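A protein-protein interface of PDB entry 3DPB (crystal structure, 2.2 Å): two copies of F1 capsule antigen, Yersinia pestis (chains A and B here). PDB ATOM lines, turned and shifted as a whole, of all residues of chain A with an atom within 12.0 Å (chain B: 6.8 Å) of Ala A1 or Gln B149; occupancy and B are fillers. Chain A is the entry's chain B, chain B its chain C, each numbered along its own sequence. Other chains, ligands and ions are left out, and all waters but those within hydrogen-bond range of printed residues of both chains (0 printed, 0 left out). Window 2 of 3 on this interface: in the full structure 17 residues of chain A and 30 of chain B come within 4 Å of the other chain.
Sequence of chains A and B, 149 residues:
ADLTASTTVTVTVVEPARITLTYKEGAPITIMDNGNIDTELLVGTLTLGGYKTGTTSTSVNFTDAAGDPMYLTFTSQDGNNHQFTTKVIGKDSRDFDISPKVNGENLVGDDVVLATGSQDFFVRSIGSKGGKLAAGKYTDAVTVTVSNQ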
ATOM      1  N   ALA A   1      -2.868 -10.102   0.381  1.00  0.00           N
ATOM      2  CA  ALA A   1      -3.501  -8.899  -0.215  1.00  0.00           C
ATOM      3  C   ALA A   1      -4.919  -9.249  -0.644  1.00  0.00           C
ATOM      4  O   ALA A   1      -5.207 -10.411  -1.018  1.00  0.00           O
ATOM      5  CB  ALA A   1      -2.721  -8.420  -1.409  1.00  0.00           C
ATOM      6  N   ASP A   2      -5.782  -8.228  -0.590  1.00  0.00           N
ATOM      7  CA  ASP A   2      -7.167  -8.327  -1.013  1.00  0.00           C
ATOM      8  C   ASP A   2      -7.312  -7.655  -2.377  1.00  0.00           C
ATOM      9  O   ASP A   2      -6.893  -6.519  -2.580  1.00  0.00           O
ATOM     10  CB  ASP A   2      -8.087  -7.678   0.034  1.00  0.00           C
ATOM     11  CG  ASP A   2      -8.024  -8.383   1.397  1.00  0.00           C
ATOM     12  OD1 ASP A   2      -8.861  -8.092   2.264  1.00  0.00           O
ATOM     13  OD2 ASP A   2      -7.136  -9.222   1.630  1.00  0.00           O
ATOM     14  N   LEU A   3      -7.875  -8.394  -3.319  1.00  0.00           N
ATOM     15  CA  LEU A   3      -8.268  -7.848  -4.612  1.00  0.00           C
ATOM     16  C   LEU A   3      -9.795  -7.891  -4.724  1.00  0.00           C
ATOM     17  O   LEU A   3     -10.447  -8.766  -4.154  1.00  0.00           O
ATOM     18  CB  LEU A   3      -7.610  -8.629  -5.761  1.00  0.00           C
ATOM     19  CG  LEU A   3      -6.064  -8.717  -5.833  1.00  0.00           C
ATOM     20  CD1 LEU A   3      -5.601  -9.532  -7.011  1.00  0.00           C
ATOM     21  CD2 LEU A   3      -5.414  -7.333  -5.865  1.00  0.00           C
ATOM     22  N   THR A   4     -10.335  -6.932  -5.471  1.00  0.00           N
ATOM     23  CA  THR A   4     -11.755  -6.735  -5.602  1.00  0.00           C
ATOM     24  C   THR A   4     -12.129  -6.501  -7.063  1.00  0.00           C
ATOM     25  O   THR A   4     -11.306  -6.068  -7.875  1.00  0.00           O
ATOM     26  CB  THR A   4     -12.252  -5.519  -4.798  1.00  0.00           C
ATOM     27  OG1 THR A   4     -11.908  -4.315  -5.495  1.00  0.00           O
ATOM     28  CG2 THR A   4     -11.639  -5.468  -3.395  1.00  0.00           C
ATOM     29  N   ALA A   5     -13.380  -6.812  -7.375  1.00  0.00           N
ATOM     30  CA  ALA A   5     -14.008  -6.452  -8.629  1.00  0.00           C
ATOM     31  C   ALA A   5     -15.499  -6.193  -8.303  1.00  0.00           C
ATOM     32  O   ALA A   5     -15.959  -6.510  -7.200  1.00  0.00           O
ATOM     33  CB  ALA A   5     -13.857  -7.580  -9.623  1.00  0.00           C
ATOM     34  N   ILE B  19      -8.363  -9.633 -10.679  1.00  0.00           N
ATOM     35  CA  ILE B  19      -9.663 -10.294 -10.321  1.00  0.00           C
ATOM     36  C   ILE B  19     -10.750  -9.769 -11.220  1.00  0.00           C
ATOM     37  O   ILE B  19     -10.838  -8.556 -11.434  1.00  0.00           O
ATOM     38  CB  ILE B  19     -10.039 -10.115  -8.812  1.00  0.00           C
ATOM     39  CG1 ILE B  19      -9.042 -10.864  -7.910  1.00  0.00           C
ATOM     40  CG2 ILE B  19     -11.453 -10.600  -8.516  1.00  0.00           C
ATOM     41  CD1 ILE B  19      -9.084 -12.405  -7.996  1.00  0.00           C
ATOM     42  N   GLY B  50      -9.393 -15.079 -11.846  1.00  0.00           N
ATOM     43  CA  GLY B  50      -8.167 -14.318 -11.692  1.00  0.00           C
ATOM     44  C   GLY B  50      -7.433 -14.571 -10.410  1.00  0.00           C
ATOM     45  O   GLY B  50      -6.355 -14.025 -10.205  1.00  0.00           O
ATOM     46  N   TYR B  51      -7.998 -15.386  -9.541  1.00  0.00           N
ATOM     47  CA  TYR B  51      -7.382 -15.616  -8.247  1.00  0.00           C
ATOM     48  C   TYR B  51      -6.207 -16.580  -8.379  1.00  0.00           C
ATOM     49  O   TYR B  51      -6.031 -17.257  -9.400  1.00  0.00           O
ATOM     50  CB  TYR B  51      -8.396 -16.161  -7.211  1.00  0.00           C
ATOM     51  CG  TYR B  51      -9.265 -17.263  -7.787  1.00  0.00           C
ATOM     52  CD1 TYR B  51      -8.804 -18.569  -7.872  1.00  0.00           C
ATOM     53  CD2 TYR B  51     -10.551 -16.971  -8.274  1.00  0.00           C
ATOM     54  CE1 TYR B  51      -9.601 -19.569  -8.437  1.00  0.00           C
ATOM     55  CE2 TYR B  51     -11.344 -17.944  -8.836  1.00  0.00           C
ATOM     56  CZ  TYR B  51     -10.864 -19.242  -8.916  1.00  0.00           C
ATOM     57  OH  TYR B  51     -11.655 -20.189  -9.479  1.00  0.00           O
ATOM     58  N   LYS B  52      -5.474 -16.660  -7.280  1.00  0.00           N
ATOM     59  CA  LYS B  52      -4.220 -17.372  -7.122  1.00  0.00           C
ATOM     60  C   LYS B  52      -4.541 -18.838  -6.996  1.00  0.00           C
ATOM     61  O   LYS B  52      -5.578 -19.188  -6.461  1.00  0.00           O
ATOM     62  CB  LYS B  52      -3.606 -16.928  -5.787  1.00  0.00           C
ATOM     63  CG  LYS B  52      -2.240 -16.304  -5.870  1.00  0.00           C
ATOM     64  CD  LYS B  52      -1.700 -15.932  -4.473  1.00  0.00           C
ATOM     65  CE  LYS B  52      -0.872 -17.066  -3.867  1.00  0.00           C
ATOM     66  NZ  LYS B  52      -0.409 -16.742  -2.478  1.00  0.00           N
ATOM     67  N   THR B  53      -3.630 -19.682  -7.469  1.00  0.00           N
ATOM     68  CA  THR B  53      -3.605 -21.123  -7.173  1.00  0.00           C
ATOM     69  C   THR B  53      -3.895 -21.405  -5.701  1.00  0.00           C
ATOM     70  O   THR B  53      -3.248 -20.858  -4.797  1.00  0.00           O
ATOM     71  CB  THR B  53      -2.200 -21.703  -7.528  1.00  0.00           C
ATOM     72  OG1 THR B  53      -1.983 -21.559  -8.937  1.00  0.00           O
ATOM     73  CG2 THR B  53      -2.050 -23.193  -7.132  1.00  0.00           C
ATOM     74  N   THR B  55      -6.607 -20.789  -3.886  1.00  0.00           N
ATOM     75  CA  THR B  55      -7.639 -19.952  -3.246  1.00  0.00           C
ATOM     76  C   THR B  55      -8.874 -20.792  -2.882  1.00  0.00           C
ATOM     77  O   THR B  55      -9.432 -21.528  -3.712  1.00  0.00           O
ATOM     78  CB  THR B  55      -8.068 -18.766  -4.144  1.00  0.00           C
ATOM     79  OG1 THR B  55      -6.925 -17.964  -4.463  1.00  0.00           O
ATOM     80  CG2 THR B  55      -9.134 -17.888  -3.439  1.00  0.00           C
ATOM     81  N   THR B  56      -9.270 -20.676  -1.621  1.00  0.00           N
ATOM     82  CA  THR B  56     -10.453 -21.350  -1.122  1.00  0.00           C
ATOM     83  C   THR B  56     -11.644 -20.375  -1.042  1.00  0.00           C
ATOM     84  O   THR B  56     -11.499 -19.165  -1.191  1.00  0.00           O
ATOM     85  CB  THR B  56     -10.202 -21.993   0.247  1.00  0.00           C
ATOM     86  OG1 THR B  56     -10.036 -20.966   1.234  1.00  0.00           O
ATOM     87  CG2 THR B  56      -8.931 -22.864   0.221  1.00  0.00           C
ATOM     88  N   SER B  59     -11.836 -17.294   1.415  1.00  0.00           N
ATOM     89  CA  SER B  59     -11.207 -16.055   0.975  1.00  0.00           C
ATOM     90  C   SER B  59     -12.068 -15.217  -0.016  1.00  0.00           C
ATOM     91  O   SER B  59     -11.684 -14.095  -0.376  1.00  0.00           O
ATOM     92  CB  SER B  59      -9.829 -16.366   0.391  1.00  0.00           C
ATOM     93  OG  SER B  59      -9.029 -17.046   1.360  1.00  0.00           O
ATOM     94  N   VAL B 146     -11.554 -10.725  -2.790  1.00  0.00           N
ATOM     95  CA  VAL B 146     -10.806 -11.969  -2.661  1.00  0.00           C
ATOM     96  C   VAL B 146      -9.525 -11.744  -1.836  1.00  0.00           C
ATOM     97  O   VAL B 146      -8.624 -10.992  -2.229  1.00  0.00           O
ATOM     98  CB  VAL B 146     -10.481 -12.604  -4.042  1.00  0.00           C
ATOM     99  CG1 VAL B 146      -9.773 -13.931  -3.850  1.00  0.00           C
ATOM    100  CG2 VAL B 146     -11.752 -12.810  -4.888  1.00  0.00           C
ATOM    101  N   SER B 147      -9.464 -12.423  -0.700  1.00  0.00           N
ATOM    102  CA  SER B 147      -8.358 -12.331   0.230  1.00  0.00           C
ATOM    103  C   SER B 147      -7.250 -13.354  -0.032  1.00  0.00           C
ATOM    104  O   SER B 147      -7.339 -14.221  -0.941  1.00  0.00           O
ATOM    105  CB  SER B 147      -8.888 -12.540   1.642  1.00  0.00           C
ATOM    106  OG  SER B 147      -9.788 -11.508   1.963  1.00  0.00           O
ATOM    107  N   ASN B 148      -6.211 -13.251   0.795  1.00  0.00           N
ATOM    108  CA  ASN B 148      -5.053 -14.152   0.762  1.00  0.00           C
ATOM    109  C   ASN B 148      -4.442 -14.261  -0.629  1.00  0.00           C
ATOM    110  O   ASN B 148      -4.029 -15.346  -1.071  1.00  0.00           O
ATOM    111  CB  ASN B 148      -5.440 -15.504   1.347  1.00  0.00           C
ATOM    112  CG  ASN B 148      -5.921 -15.384   2.772  1.00  0.00           C
ATOM    113  OD1 ASN B 148      -5.185 -14.937   3.634  1.00  0.00           O
ATOM    114  ND2 ASN B 148      -7.158 -15.759   3.025  1.00  0.00           N
ATOM    115  N   GLN B 149      -4.410 -13.127  -1.328  1.00  0.00           N
ATOM    116  CA  GLN B 149      -3.843 -13.084  -2.667  1.00  0.00           C
ATOM    117  C   GLN B 149      -2.380 -12.604  -2.626  1.00  0.00           C
ATOM    118  O   GLN B 149      -1.777 -12.403  -3.701  1.00  0.00           O
ATOM    119  CB  GLN B 149      -4.698 -12.225  -3.623  1.00  0.00           C
ATOM    120  CG  GLN B 149      -6.171 -12.724  -3.817  1.00  0.00           C
ATOM    121  CD  GLN B 149      -6.256 -14.128  -4.373  1.00  0.00           C
ATOM    122  OE1 GLN B 149      -5.931 -14.377  -5.542  1.00  0.00           O
ATOM    123  NE2 GLN B 149      -6.689 -15.056  -3.546  1.00  0.00           N
ATOM    124  OXT GLN B 149      -1.773 -12.433  -1.544  1.00  0.00           O
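Of the 5 printed residues of chain A, 4 touch a printed residue of chain B.
Printed residues of chain B that touch a printed residue of chain A: Ile B19, Val B146, Ser B147, Asn B148 and Gln B149.
Among the printed residues, no Asp or Glu carboxylate lies within 4 Å of a Lys or Arg side-chain nitrogen of the other chain.
No position is printed for both chains.
Of the 9 pairs that touch across the chains among the printed residues, none has its exchanged pair printed and touching as well.
The backbone carbonyl oxygen (O) of Ala A1 is in hydrogen-bond range of the backbone NH (N) of Gln B149, 2.8 Å away.
N of Val B146 sits at hydrogen-bond distance from O of Leu A3, 2.6 Å away.
N of Lys B52 sits at hydrogen-bond distance from OE1 of Gln B149, 2.9 Å away.
OG1 of Thr B55 lies within hydrogen-bond range of NE2 of Gln B149, at 3.1 Å.
The backbone carbonyl oxygen of Ser B59 sits at hydrogen-bond distance from the backbone NH of Ser B147.
OG of Ser B59 lies within hydrogen-bond range of ND2 of Asn B148 (2.8 Å).
The side-chain amide nitrogen of Gln B149 lies within hydrogen-bond range of the backbone carbonyl oxygen of Ser B147 (2.8 Å).
Ala A1 touches just these residues of chain B: Val B146, Ser B147, Asn B148 and Gln B149.
Of the printed residues of chain B, Asp A2 touches Val B146 and Ser B147.
Of the printed residues of chain B, Leu A3 touches Ile B19 and Val B146.
Thr A4 touches none of the printed residues of chain B.
Of the printed residues of chain B, Ala A5 touches Ile B19 (3.7 Å).
Of the printed residues of chain A, Ile B19 touches Leu A3 and Ala A5.
No residue of chain A comes within 4 Å of Gly B50.
Tyr B51 touches none of the printed residues of chain A.
Thr B55 touches none of the printed residues of chain A.
No residue of chain A comes within 4 Å of Ser B59.
Printed residues of chain A within 4 Å of Val B146: Ala A1, Asp A2 and Leu A3.
Ser B147 touches just these residues of chain A: Ala A1 and Asp A2.
Asn B148 touches one residue of chain A.
The nearest printed residue of chain B that does not touch Ala A1 is Lys B52 (7.4 Å).
The nearest residue of chain A that does not touch Gln B149 is Leu A3 (4.4 Å).
Among the printed residues, pairs that only touch across the chains: Ala A1 with Val B146, Ala A1 with Ser B147, Ala A1 with Asn B148, Asp A2 with Val B146, Asp A2 with Ser B147, Leu A3 with Ile B19 and Ala A5 with Ile B19.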
